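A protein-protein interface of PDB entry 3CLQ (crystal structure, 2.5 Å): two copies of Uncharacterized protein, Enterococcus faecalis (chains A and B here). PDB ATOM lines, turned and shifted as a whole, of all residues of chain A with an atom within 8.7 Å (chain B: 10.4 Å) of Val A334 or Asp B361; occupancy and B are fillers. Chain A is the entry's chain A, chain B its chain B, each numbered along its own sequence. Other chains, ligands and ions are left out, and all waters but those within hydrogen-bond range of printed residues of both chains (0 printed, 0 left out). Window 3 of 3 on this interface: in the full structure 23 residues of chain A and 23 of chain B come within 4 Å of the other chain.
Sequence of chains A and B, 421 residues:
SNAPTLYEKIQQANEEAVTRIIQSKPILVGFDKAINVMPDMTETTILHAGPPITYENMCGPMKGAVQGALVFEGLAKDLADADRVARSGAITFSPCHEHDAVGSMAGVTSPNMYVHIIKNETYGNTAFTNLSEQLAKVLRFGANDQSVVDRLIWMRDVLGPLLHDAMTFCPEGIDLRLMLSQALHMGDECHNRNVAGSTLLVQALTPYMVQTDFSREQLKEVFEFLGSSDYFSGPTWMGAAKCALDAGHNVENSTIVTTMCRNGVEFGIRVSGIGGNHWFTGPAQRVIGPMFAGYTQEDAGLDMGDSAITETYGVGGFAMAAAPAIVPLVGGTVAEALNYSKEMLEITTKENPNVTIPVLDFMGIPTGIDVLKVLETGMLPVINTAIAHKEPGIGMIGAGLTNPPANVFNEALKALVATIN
The side-chain hydroxyl (OG1) of Thr B356 is in hydrogen-bond range of a ring nitrogen (NE2) of His B185.
The backbone carbonyl oxygen (O) of Ile B357 lies within hydrogen-bond range of the backbone NH (N) of Phe B362.
Of the 20 printed residues of chain B, 5 touch a printed residue of chain A.
Of the 22 printed residues of chain A, 4 touch a printed residue of chain B.
Hydrophobic or aromatic side chains of chain A within 4 Å of the printed part of chain B: Pro A324, Ala A325, Pro A328 and Val A334.
Along chain A the printed residues that touch a printed residue of chain B span positions 324 to 334.
Among the printed residues, no Asp or Glu carboxylate lies within 4 Å of a Lys or Arg side-chain nitrogen of the other chain.
Positions printed for both chains: 321, 322, 338, 341, 342 and 359.
Of the 7 pairs that touch across the chains among the printed residues, none has its exchanged pair printed and touching as well.
Among the printed residues, merely in contact across the chains: Pro A324 with Pro B358 (3.9 Å), Pro A324 with Phe B362 (3.9 Å), Ala A325 with His B185 (3.8 Å), Pro A328 with Phe B362 (3.4 Å), Val A334 with Pro B358 (3.7 Å), Val A334 with Val B359 (3.6 Å) and Val A334 with Asp B361 (3.9 Å).
Val A334 touches three residues of chain B.
Asp B361 touches just one residue of chain A: Val A334 (3.9 Å).
Ala A335 touches none of the printed residues of chain B.
No residue of chain B comes within 4 Å of Ala A337.
No residue of chain B comes within 4 Å of Leu A338.
Printed residues of chain B within 4 Å of Ala A325: His B185.
Printed residues of chain A within 4 Å of Pro B358: Pro A324 and Val A334.
Of the printed residues of chain A, His B185 touches Ala A325 (3.8 Å).
Of the printed residues of chain B, Pro A324 touches Pro B358 and Phe B362.
Of the printed residues of chain A, Phe B362 touches Pro A324 (3.9 Å) and Pro A328 (3.4 Å).
The nearest residue of chain A that does not touch Asp B361 is Thr A333 (4.6 Å).
The nearest printed residue of chain A that does not touch Val B359 is Pro A324 (4.1 Å).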
ATOM      1  N   MET A 320      23.623 -34.234 -14.089  1.00  0.00           N
ATOM      2  CA  MET A 320      24.456 -33.190 -14.689  1.00  0.00           C
ATOM      3  C   MET A 320      24.037 -31.750 -14.419  1.00  0.00           C
ATOM      4  O   MET A 320      24.850 -30.833 -14.557  1.00  0.00           O
ATOM      5  CB  MET A 320      24.685 -33.404 -16.177  1.00  0.00           C
ATOM      6  CG  MET A 320      25.943 -34.246 -16.462  1.00  0.00           C
ATOM      7  SD  MET A 320      26.077 -34.607 -18.379  1.00  0.00           S
ATOM      8  CE  MET A 320      25.788 -32.806 -19.044  1.00  0.00           C
ATOM      9  N   ALA A 321      22.793 -31.535 -14.016  1.00  0.00           N
ATOM     10  CA  ALA A 321      22.360 -30.172 -13.737  1.00  0.00           C
ATOM     11  C   ALA A 321      23.112 -29.615 -12.518  1.00  0.00           C
ATOM     12  O   ALA A 321      23.262 -28.402 -12.366  1.00  0.00           O
ATOM     13  CB  ALA A 321      20.858 -30.126 -13.516  1.00  0.00           C
ATOM     14  N   ALA A 322      23.605 -30.524 -11.681  1.00  0.00           N
ATOM     15  CA  ALA A 322      24.228 -30.172 -10.428  1.00  0.00           C
ATOM     16  C   ALA A 322      25.631 -29.642 -10.700  1.00  0.00           C
ATOM     17  O   ALA A 322      26.210 -28.898  -9.903  1.00  0.00           O
ATOM     18  CB  ALA A 322      24.279 -31.400  -9.511  1.00  0.00           C
ATOM     19  N   ALA A 323      26.146 -29.995 -11.870  1.00  0.00           N
ATOM     20  CA  ALA A 323      27.557 -29.853 -12.165  1.00  0.00           C
ATOM     21  C   ALA A 323      27.774 -29.127 -13.455  1.00  0.00           C
ATOM     22  O   ALA A 323      28.447 -29.646 -14.313  1.00  0.00           O
ATOM     23  CB  ALA A 323      28.213 -31.257 -12.252  1.00  0.00           C
ATOM     24  N   PRO A 324      27.242 -27.911 -13.598  1.00  0.00           N
ATOM     25  CA  PRO A 324      27.429 -27.247 -14.883  1.00  0.00           C
ATOM     26  C   PRO A 324      28.900 -27.093 -15.249  1.00  0.00           C
ATOM     27  O   PRO A 324      29.223 -26.781 -16.389  1.00  0.00           O
ATOM     28  CB  PRO A 324      26.822 -25.861 -14.652  1.00  0.00           C
ATOM     29  CG  PRO A 324      26.872 -25.662 -13.163  1.00  0.00           C
ATOM     30  CD  PRO A 324      26.534 -27.048 -12.646  1.00  0.00           C
ATOM     31  N   ALA A 325      29.796 -27.292 -14.293  1.00  0.00           N
ATOM     32  CA  ALA A 325      31.213 -27.093 -14.571  1.00  0.00           C
ATOM     33  C   ALA A 325      31.845 -28.144 -15.501  1.00  0.00           C
ATOM     34  O   ALA A 325      32.877 -27.852 -16.096  1.00  0.00           O
ATOM     35  CB  ALA A 325      32.003 -26.961 -13.288  1.00  0.00           C
ATOM     36  N   ILE A 326      31.255 -29.341 -15.642  1.00  0.00           N
ATOM     37  CA  ILE A 326      31.809 -30.312 -16.610  1.00  0.00           C
ATOM     38  C   ILE A 326      31.514 -30.062 -18.084  1.00  0.00           C
ATOM     39  O   ILE A 326      31.872 -30.875 -18.930  1.00  0.00           O
ATOM     40  CB  ILE A 326      31.327 -31.729 -16.417  1.00  0.00           C
ATOM     41  CG1 ILE A 326      29.817 -31.831 -16.534  1.00  0.00           C
ATOM     42  CG2 ILE A 326      31.764 -32.290 -15.136  1.00  0.00           C
ATOM     43  CD1 ILE A 326      29.400 -33.278 -16.272  1.00  0.00           C
ATOM     44  N   VAL A 327      30.836 -28.984 -18.411  1.00  0.00           N
ATOM     45  CA  VAL A 327      30.425 -28.823 -19.778  1.00  0.00           C
ATOM     46  C   VAL A 327      31.627 -28.758 -20.739  1.00  0.00           C
ATOM     47  O   VAL A 327      31.705 -29.568 -21.651  1.00  0.00           O
ATOM     48  CB  VAL A 327      29.356 -27.712 -19.908  1.00  0.00           C
ATOM     49  CG1 VAL A 327      29.356 -27.036 -21.283  1.00  0.00           C
ATOM     50  CG2 VAL A 327      27.990 -28.317 -19.557  1.00  0.00           C
ATOM     51  N   PRO A 328      32.595 -27.845 -20.516  1.00  0.00           N
ATOM     52  CA  PRO A 328      33.804 -27.866 -21.361  1.00  0.00           C
ATOM     53  C   PRO A 328      34.454 -29.248 -21.473  1.00  0.00           C
ATOM     54  O   PRO A 328      34.898 -29.606 -22.552  1.00  0.00           O
ATOM     55  CB  PRO A 328      34.757 -26.902 -20.640  1.00  0.00           C
ATOM     56  CG  PRO A 328      34.152 -26.694 -19.274  1.00  0.00           C
ATOM     57  CD  PRO A 328      32.675 -26.773 -19.513  1.00  0.00           C
ATOM     58  N   GLY A 331      31.215 -31.615 -23.431  1.00  0.00           N
ATOM     59  CA  GLY A 331      30.514 -31.178 -24.624  1.00  0.00           C
ATOM     60  C   GLY A 331      29.121 -30.690 -24.287  1.00  0.00           C
ATOM     61  O   GLY A 331      28.598 -30.992 -23.204  1.00  0.00           O
ATOM     62  N   GLY A 332      28.528 -29.927 -25.200  1.00  0.00           N
ATOM     63  CA  GLY A 332      27.154 -29.463 -25.060  1.00  0.00           C
ATOM     64  C   GLY A 332      27.028 -28.089 -24.419  1.00  0.00           C
ATOM     65  O   GLY A 332      28.038 -27.488 -24.034  1.00  0.00           O
ATOM     66  N   THR A 333      25.791 -27.604 -24.299  1.00  0.00           N
ATOM     67  CA  THR A 333      25.499 -26.377 -23.568  1.00  0.00           C
ATOM     68  C   THR A 333      25.279 -26.658 -22.087  1.00  0.00           C
ATOM     69  O   THR A 333      25.137 -27.822 -21.693  1.00  0.00           O
ATOM     70  CB  THR A 333      24.216 -25.727 -24.074  1.00  0.00           C
ATOM     71  OG1 THR A 333      23.881 -26.286 -25.344  1.00  0.00           O
ATOM     72  CG2 THR A 333      24.409 -24.173 -24.225  1.00  0.00           C
ATOM     73  N   VAL A 334      25.231 -25.612 -21.254  1.00  0.00           N
ATOM     74  CA  VAL A 334      24.775 -25.842 -19.876  1.00  0.00           C
ATOM     75  C   VAL A 334      23.235 -26.014 -19.873  1.00  0.00           C
ATOM     76  O   VAL A 334      22.709 -26.886 -19.178  1.00  0.00           O
ATOM     77  CB  VAL A 334      25.297 -24.801 -18.813  1.00  0.00           C
ATOM     78  CG1 VAL A 334      26.671 -24.267 -19.172  1.00  0.00           C
ATOM     79  CG2 VAL A 334      24.321 -23.684 -18.612  1.00  0.00           C
ATOM     80  N   ALA A 335      22.537 -25.227 -20.687  1.00  0.00           N
ATOM     81  CA  ALA A 335      21.111 -25.466 -20.955  1.00  0.00           C
ATOM     82  C   ALA A 335      20.761 -26.963 -21.025  1.00  0.00           C
ATOM     83  O   ALA A 335      19.937 -27.441 -20.248  1.00  0.00           O
ATOM     84  CB  ALA A 335      20.675 -24.754 -22.238  1.00  0.00           C
ATOM     85  N   GLU A 336      21.401 -27.690 -21.941  1.00  0.00           N
ATOM     86  CA  GLU A 336      21.173 -29.112 -22.108  1.00  0.00           C
ATOM     87  C   GLU A 336      21.554 -29.880 -20.863  1.00  0.00           C
ATOM     88  O   GLU A 336      20.880 -30.829 -20.477  1.00  0.00           O
ATOM     89  CB  GLU A 336      22.016 -29.659 -23.263  1.00  0.00           C
ATOM     90  CG  GLU A 336      21.760 -29.044 -24.679  1.00  0.00           C
ATOM     91  CD  GLU A 336      22.886 -29.413 -25.688  1.00  0.00           C
ATOM     92  OE1 GLU A 336      23.885 -30.042 -25.257  1.00  0.00           O
ATOM     93  OE2 GLU A 336      22.788 -29.084 -26.903  1.00  0.00           O
ATOM     94  N   ALA A 337      22.664 -29.501 -20.246  1.00  0.00           N
ATOM     95  CA  ALA A 337      23.100 -30.177 -19.036  1.00  0.00           C
ATOM     96  C   ALA A 337      22.061 -30.031 -17.932  1.00  0.00           C
ATOM     97  O   ALA A 337      21.909 -30.934 -17.123  1.00  0.00           O
ATOM     98  CB  ALA A 337      24.437 -29.662 -18.572  1.00  0.00           C
ATOM     99  N   LEU A 338      21.340 -28.913 -17.891  1.00  0.00           N
ATOM    100  CA  LEU A 338      20.281 -28.747 -16.898  1.00  0.00           C
ATOM    101  C   LEU A 338      19.095 -29.597 -17.303  1.00  0.00           C
ATOM    102  O   LEU A 338      18.328 -30.090 -16.475  1.00  0.00           O
ATOM    103  CB  LEU A 338      19.819 -27.286 -16.791  1.00  0.00           C
ATOM    104  CG  LEU A 338      20.821 -26.255 -16.260  1.00  0.00           C
ATOM    105  CD1 LEU A 338      20.125 -24.910 -16.096  1.00  0.00           C
ATOM    106  CD2 LEU A 338      21.503 -26.688 -14.961  1.00  0.00           C
ATOM    107  N   ASN A 339      18.940 -29.779 -18.592  1.00  0.00           N
ATOM    108  CA  ASN A 339      17.775 -30.468 -19.032  1.00  0.00           C
ATOM    109  C   ASN A 339      17.818 -31.972 -18.772  1.00  0.00           C
ATOM    110  O   ASN A 339      16.777 -32.587 -18.525  1.00  0.00           O
ATOM    111  CB  ASN A 339      17.551 -30.195 -20.495  1.00  0.00           C
ATOM    112  CG  ASN A 339      16.131 -29.909 -20.783  1.00  0.00           C
ATOM    113  OD1 ASN A 339      15.473 -29.194 -20.015  1.00  0.00           O
ATOM    114  ND2 ASN A 339      15.615 -30.474 -21.881  1.00  0.00           N
ATOM    115  N   TYR A 340      19.002 -32.573 -18.830  1.00  0.00           N
ATOM    116  CA  TYR A 340      19.052 -34.026 -18.795  1.00  0.00           C
ATOM    117  C   TYR A 340      18.446 -34.563 -17.512  1.00  0.00           C
ATOM    118  O   TYR A 340      17.697 -35.543 -17.520  1.00  0.00           O
ATOM    119  CB  TYR A 340      20.469 -34.565 -18.900  1.00  0.00           C
ATOM    120  CG  TYR A 340      21.158 -34.350 -20.215  1.00  0.00           C
ATOM    121  CD1 TYR A 340      20.555 -34.698 -21.427  1.00  0.00           C
ATOM    122  CD2 TYR A 340      22.460 -33.845 -20.233  1.00  0.00           C
ATOM    123  CE1 TYR A 340      21.229 -34.503 -22.629  1.00  0.00           C
ATOM    124  CE2 TYR A 340      23.131 -33.640 -21.413  1.00  0.00           C
ATOM    125  CZ  TYR A 340      22.527 -33.960 -22.602  1.00  0.00           C
ATOM    126  OH  TYR A 340      23.262 -33.714 -23.731  1.00  0.00           O
ATOM    127  N   SER A 341      18.794 -33.938 -16.400  1.00  0.00           N
ATOM    128  CA  SER A 341      18.273 -34.401 -15.134  1.00  0.00           C
ATOM    129  C   SER A 341      16.761 -34.293 -15.122  1.00  0.00           C
ATOM    130  O   SER A 341      16.094 -35.142 -14.538  1.00  0.00           O
ATOM    131  CB  SER A 341      18.879 -33.616 -13.998  1.00  0.00           C
ATOM    132  OG  SER A 341      20.287 -33.660 -14.125  1.00  0.00           O
ATOM    133  N   LYS A 342      16.216 -33.273 -15.789  1.00  0.00           N
ATOM    134  CA  LYS A 342      14.771 -33.114 -15.795  1.00  0.00           C
ATOM    135  C   LYS A 342      14.161 -34.180 -16.675  1.00  0.00           C
ATOM    136  O   LYS A 342      13.124 -34.732 -16.362  1.00  0.00           O
ATOM    137  CB  LYS A 342      14.342 -31.730 -16.270  1.00  0.00           C
ATOM    138  CG  LYS A 342      14.368 -30.644 -15.221  1.00  0.00           C
ATOM    139  CD  LYS A 342      13.470 -29.480 -15.640  1.00  0.00           C
ATOM    140  CE  LYS A 342      13.961 -28.101 -15.128  1.00  0.00           C
ATOM    141  NZ  LYS A 342      15.011 -27.479 -16.024  1.00  0.00           N
ATOM    142  N   VAL A 359      20.054 -26.260  -8.083  1.00  0.00           N
ATOM    143  CA  VAL A 359      19.650 -25.397  -9.184  1.00  0.00           C
ATOM    144  C   VAL A 359      18.256 -25.807  -9.659  1.00  0.00           C
ATOM    145  O   VAL A 359      17.538 -25.021 -10.306  1.00  0.00           O
ATOM    146  CB  VAL A 359      20.659 -25.446 -10.353  1.00  0.00           C
ATOM    147  CG1 VAL A 359      20.452 -26.702 -11.186  1.00  0.00           C
ATOM    148  CG2 VAL A 359      20.585 -24.146 -11.208  1.00  0.00           C
ATOM    149  N   HIS B 185      33.482 -22.762  -9.080  1.00  0.00           N
ATOM    150  CA  HIS B 185      32.953 -23.786  -9.955  1.00  0.00           C
ATOM    151  C   HIS B 185      32.428 -24.908  -9.093  1.00  0.00           C
ATOM    152  O   HIS B 185      31.960 -25.898  -9.621  1.00  0.00           O
ATOM    153  CB  HIS B 185      34.021 -24.292 -10.914  1.00  0.00           C
ATOM    154  CG  HIS B 185      34.258 -23.383 -12.077  1.00  0.00           C
ATOM    155  ND1 HIS B 185      34.936 -23.778 -13.206  1.00  0.00           N
ATOM    156  CD2 HIS B 185      33.891 -22.100 -12.295  1.00  0.00           C
ATOM    157  CE1 HIS B 185      34.992 -22.776 -14.060  1.00  0.00           C
ATOM    158  NE2 HIS B 185      34.370 -21.746 -13.531  1.00  0.00           N
ATOM    159  N   ALA B 321      24.735 -16.276  -8.562  1.00  0.00           N
ATOM    160  CA  ALA B 321      24.334 -17.343  -9.489  1.00  0.00           C
ATOM    161  C   ALA B 321      25.118 -18.641  -9.358  1.00  0.00           C
ATOM    162  O   ALA B 321      24.614 -19.705  -9.690  1.00  0.00           O
ATOM    163  CB  ALA B 321      24.416 -16.858 -10.920  1.00  0.00           C
ATOM    164  N   ALA B 322      26.355 -18.543  -8.904  1.00  0.00           N
ATOM    165  CA  ALA B 322      27.262 -19.683  -8.821  1.00  0.00           C
ATOM    166  C   ALA B 322      26.910 -20.615  -7.668  1.00  0.00           C
ATOM    167  O   ALA B 322      27.416 -21.727  -7.591  1.00  0.00           O
ATOM    168  CB  ALA B 322      28.671 -19.198  -8.649  1.00  0.00           C
ATOM    169  N   LEU B 338      20.255 -15.922 -10.648  1.00  0.00           N
ATOM    170  CA  LEU B 338      20.875 -15.898 -11.966  1.00  0.00           C
ATOM    171  C   LEU B 338      20.799 -14.479 -12.460  1.00  0.00           C
ATOM    172  O   LEU B 338      21.745 -13.937 -12.997  1.00  0.00           O
ATOM    173  CB  LEU B 338      20.119 -16.792 -12.949  1.00  0.00           C
ATOM    174  CG  LEU B 338      20.034 -18.273 -12.583  1.00  0.00           C
ATOM    175  CD1 LEU B 338      19.507 -19.133 -13.747  1.00  0.00           C
ATOM    176  CD2 LEU B 338      21.390 -18.760 -12.106  1.00  0.00           C
ATOM    177  N   SER B 341      23.337 -11.558 -10.920  1.00  0.00           N
ATOM    178  CA  SER B 341      24.698 -11.637 -11.397  1.00  0.00           C
ATOM    179  C   SER B 341      24.792 -11.040 -12.791  1.00  0.00           C
ATOM    180  O   SER B 341      25.764 -10.332 -13.072  1.00  0.00           O
ATOM    181  CB  SER B 341      25.185 -13.078 -11.390  1.00  0.00           C
ATOM    182  OG  SER B 341      25.524 -13.476 -10.080  1.00  0.00           O
ATOM    183  N   LYS B 342      23.793 -11.312 -13.648  1.00  0.00           N
ATOM    184  CA  LYS B 342      23.687 -10.658 -14.958  1.00  0.00           C
ATOM    185  C   LYS B 342      23.536  -9.152 -14.794  1.00  0.00           C
ATOM    186  O   LYS B 342      24.245  -8.380 -15.422  1.00  0.00           O
ATOM    187  CB  LYS B 342      22.477 -11.148 -15.732  1.00  0.00           C
ATOM    188  CG  LYS B 342      22.622 -12.475 -16.438  1.00  0.00           C
ATOM    189  CD  LYS B 342      21.290 -12.791 -17.164  1.00  0.00           C
ATOM    190  CE  LYS B 342      21.218 -14.231 -17.708  1.00  0.00           C
ATOM    191  NZ  LYS B 342      20.872 -15.276 -16.677  1.00  0.00           N
ATOM    192  N   GLU B 351      34.084  -8.002 -17.313  1.00  0.00           N
ATOM    193  CA  GLU B 351      34.142  -9.349 -16.703  1.00  0.00           C
ATOM    194  C   GLU B 351      35.585  -9.769 -16.443  1.00  0.00           C
ATOM    195  O   GLU B 351      36.454  -9.583 -17.278  1.00  0.00           O
ATOM    196  CB  GLU B 351      33.512 -10.415 -17.617  1.00  0.00           C
ATOM    197  CG  GLU B 351      32.134 -10.089 -18.163  1.00  0.00           C
ATOM    198  CD  GLU B 351      31.569 -11.195 -19.079  1.00  0.00           C
ATOM    199  OE1 GLU B 351      32.164 -12.302 -19.161  1.00  0.00           O
ATOM    200  OE2 GLU B 351      30.518 -10.950 -19.727  1.00  0.00           O
ATOM    201  N   ASN B 352      35.843 -10.351 -15.282  1.00  0.00           N
ATOM    202  CA  ASN B 352      37.129 -10.976 -15.032  1.00  0.00           C
ATOM    203  C   ASN B 352      37.195 -12.361 -15.702  1.00  0.00           C
ATOM    204  O   ASN B 352      36.531 -13.292 -15.258  1.00  0.00           O
ATOM    205  CB  ASN B 352      37.306 -11.114 -13.529  1.00  0.00           C
ATOM    206  CG  ASN B 352      38.626 -11.704 -13.162  1.00  0.00           C
ATOM    207  OD1 ASN B 352      39.367 -12.178 -14.029  1.00  0.00           O
ATOM    208  ND2 ASN B 352      38.951 -11.681 -11.877  1.00  0.00           N
ATOM    209  N   PRO B 353      38.001 -12.514 -16.765  1.00  0.00           N
ATOM    210  CA  PRO B 353      38.037 -13.835 -17.440  1.00  0.00           C
ATOM    211  C   PRO B 353      38.679 -14.977 -16.612  1.00  0.00           C
ATOM    212  O   PRO B 353      38.426 -16.162 -16.866  1.00  0.00           O
ATOM    213  CB  PRO B 353      38.846 -13.562 -18.717  1.00  0.00           C
ATOM    214  CG  PRO B 353      39.685 -12.380 -18.406  1.00  0.00           C
ATOM    215  CD  PRO B 353      38.900 -11.532 -17.403  1.00  0.00           C
ATOM    216  N   VAL B 355      38.103 -15.719 -13.575  1.00  0.00           N
ATOM    217  CA  VAL B 355      37.172 -16.201 -12.553  1.00  0.00           C
ATOM    218  C   VAL B 355      35.746 -16.164 -13.111  1.00  0.00           C
ATOM    219  O   VAL B 355      35.178 -15.089 -13.332  1.00  0.00           O
ATOM    220  CB  VAL B 355      37.240 -15.324 -11.291  1.00  0.00           C
ATOM    221  CG1 VAL B 355      36.332 -15.859 -10.185  1.00  0.00           C
ATOM    222  CG2 VAL B 355      38.652 -15.209 -10.824  1.00  0.00           C
ATOM    223  N   THR B 356      35.162 -17.328 -13.339  1.00  0.00           N
ATOM    224  CA  THR B 356      33.957 -17.385 -14.124  1.00  0.00           C
ATOM    225  C   THR B 356      32.812 -18.163 -13.448  1.00  0.00           C
ATOM    226  O   THR B 356      33.047 -18.963 -12.554  1.00  0.00           O
ATOM    227  CB  THR B 356      34.288 -18.009 -15.492  1.00  0.00           C
ATOM    228  OG1 THR B 356      34.847 -19.306 -15.290  1.00  0.00           O
ATOM    229  CG2 THR B 356      35.324 -17.152 -16.243  1.00  0.00           C
ATOM    230  N   ILE B 357      31.577 -17.938 -13.896  1.00  0.00           N
ATOM    231  CA  ILE B 357      30.407 -18.623 -13.347  1.00  0.00           C
ATOM    232  C   ILE B 357      29.787 -19.585 -14.340  1.00  0.00           C
ATOM    233  O   ILE B 357      29.167 -19.178 -15.320  1.00  0.00           O
ATOM    234  CB  ILE B 357      29.320 -17.628 -12.976  1.00  0.00           C
ATOM    235  CG1 ILE B 357      29.866 -16.545 -12.024  1.00  0.00           C
ATOM    236  CG2 ILE B 357      28.132 -18.354 -12.366  1.00  0.00           C
ATOM    237  CD1 ILE B 357      29.034 -15.310 -12.062  1.00  0.00           C
ATOM    238  N   PRO B 358      29.917 -20.885 -14.076  1.00  0.00           N
ATOM    239  CA  PRO B 358      29.516 -21.921 -15.017  1.00  0.00           C
ATOM    240  C   PRO B 358      28.068 -21.772 -15.504  1.00  0.00           C
ATOM    241  O   PRO B 358      27.817 -21.684 -16.714  1.00  0.00           O
ATOM    242  CB  PRO B 358      29.676 -23.191 -14.196  1.00  0.00           C
ATOM    243  CG  PRO B 358      30.766 -22.856 -13.257  1.00  0.00           C
ATOM    244  CD  PRO B 358      30.459 -21.463 -12.841  1.00  0.00           C
ATOM    245  N   VAL B 359      27.120 -21.732 -14.578  1.00  0.00           N
ATOM    246  CA  VAL B 359      25.725 -21.712 -15.010  1.00  0.00           C
ATOM    247  C   VAL B 359      25.408 -20.537 -15.964  1.00  0.00           C
ATOM    248  O   VAL B 359      24.519 -20.640 -16.789  1.00  0.00           O
ATOM    249  CB  VAL B 359      24.734 -21.782 -13.818  1.00  0.00           C
ATOM    250  CG1 VAL B 359      24.676 -20.460 -13.098  1.00  0.00           C
ATOM    251  CG2 VAL B 359      23.353 -22.234 -14.301  1.00  0.00           C
ATOM    252  N   LEU B 360      26.140 -19.432 -15.857  1.00  0.00           N
ATOM    253  CA  LEU B 360      25.985 -18.333 -16.825  1.00  0.00           C
ATOM    254  C   LEU B 360      26.969 -18.462 -17.998  1.00  0.00           C
ATOM    255  O   LEU B 360      27.670 -17.501 -18.343  1.00  0.00           O
ATOM    256  CB  LEU B 360      26.178 -16.988 -16.133  1.00  0.00           C
ATOM    257  CG  LEU B 360      24.950 -16.302 -15.512  1.00  0.00           C
ATOM    258  CD1 LEU B 360      23.668 -17.165 -15.541  1.00  0.00           C
ATOM    259  CD2 LEU B 360      25.245 -15.786 -14.123  1.00  0.00           C
ATOM    260  N   ASP B 361      27.036 -19.662 -18.580  1.00  0.00           N
ATOM    261  CA  ASP B 361      27.916 -19.934 -19.715  1.00  0.00           C
ATOM    262  C   ASP B 361      29.348 -19.445 -19.478  1.00  0.00           C
ATOM    263  O   ASP B 361      30.021 -19.003 -20.415  1.00  0.00           O
ATOM    264  CB  ASP B 361      27.369 -19.273 -20.989  1.00  0.00           C
ATOM    265  CG  ASP B 361      26.012 -19.827 -21.417  1.00  0.00           C
ATOM    266  OD1 ASP B 361      25.744 -21.040 -21.188  1.00  0.00           O
ATOM    267  OD2 ASP B 361      25.222 -19.045 -22.010  1.00  0.00           O
ATOM    268  N   PHE B 362      29.807 -19.509 -18.229  1.00  0.00           N
ATOM    269  CA  PHE B 362      31.160 -19.069 -17.888  1.00  0.00           C
ATOM    270  C   PHE B 362      31.431 -17.589 -18.184  1.00  0.00           C
ATOM    271  O   PHE B 362      32.495 -17.260 -18.721  1.00  0.00           O
ATOM    272  CB  PHE B 362      32.196 -19.942 -18.611  1.00  0.00           C
ATOM    273  CG  PHE B 362      32.045 -21.379 -18.312  1.00  0.00           C
ATOM    274  CD1 PHE B 362      32.771 -21.965 -17.273  1.00  0.00           C
ATOM    275  CD2 PHE B 362      31.124 -22.150 -19.019  1.00  0.00           C
ATOM    276  CE1 PHE B 362      32.606 -23.304 -16.979  1.00  0.00           C
ATOM    277  CE2 PHE B 362      30.941 -23.496 -18.728  1.00  0.00           C
ATOM    278  CZ  PHE B 362      31.673 -24.078 -17.703  1.00  0.00           C
ATOM    279  N   MET B 363      30.492 -16.700 -17.851  1.00  0.00           N
ATOM    280  CA  MET B 363      30.818 -15.281 -17.896  1.00  0.00           C
ATOM    281  C   MET B 363      31.784 -14.993 -16.759  1.00  0.00           C
ATOM    282  O   MET B 363      31.746 -15.656 -15.733  1.00  0.00           O
ATOM    283  CB  MET B 363      29.572 -14.377 -17.840  1.00  0.00           C
ATOM    284  CG  MET B 363      28.903 -14.294 -16.497  1.00  0.00           C
ATOM    285  SD  MET B 363      27.720 -12.729 -16.178  1.00  0.00           S
ATOM    286  CE  MET B 363      27.871 -12.614 -14.249  1.00  0.00           C
ATOM    287  N   GLY B 364      32.683 -14.042 -16.961  1.00  0.00           N
ATOM    288  CA  GLY B 364      33.601 -13.638 -15.911  1.00  0.00           C
ATOM    289  C   GLY B 364      32.811 -12.867 -14.876  1.00  0.00           C
ATOM    290  O   GLY B 364      31.850 -12.167 -15.198  1.00  0.00           O
ATOM    291  N   ILE B 365      33.187 -12.994 -13.617  1.00  0.00           N
ATOM    292  CA  ILE B 365      32.509 -12.242 -12.589  1.00  0.00           C
ATOM    293  C   ILE B 365      32.517 -10.741 -12.929  1.00  0.00           C
ATOM    294  O   ILE B 365      33.426 -10.274 -13.619  1.00  0.00           O
ATOM    295  CB  ILE B 365      33.149 -12.501 -11.264  1.00  0.00           C
ATOM    296  CG1 ILE B 365      34.663 -12.303 -11.375  1.00  0.00           C
ATOM    297  CG2 ILE B 365      32.863 -13.913 -10.866  1.00  0.00           C
ATOM    298  CD1 ILE B 365      35.369 -12.200 -10.029  1.00  0.00           C
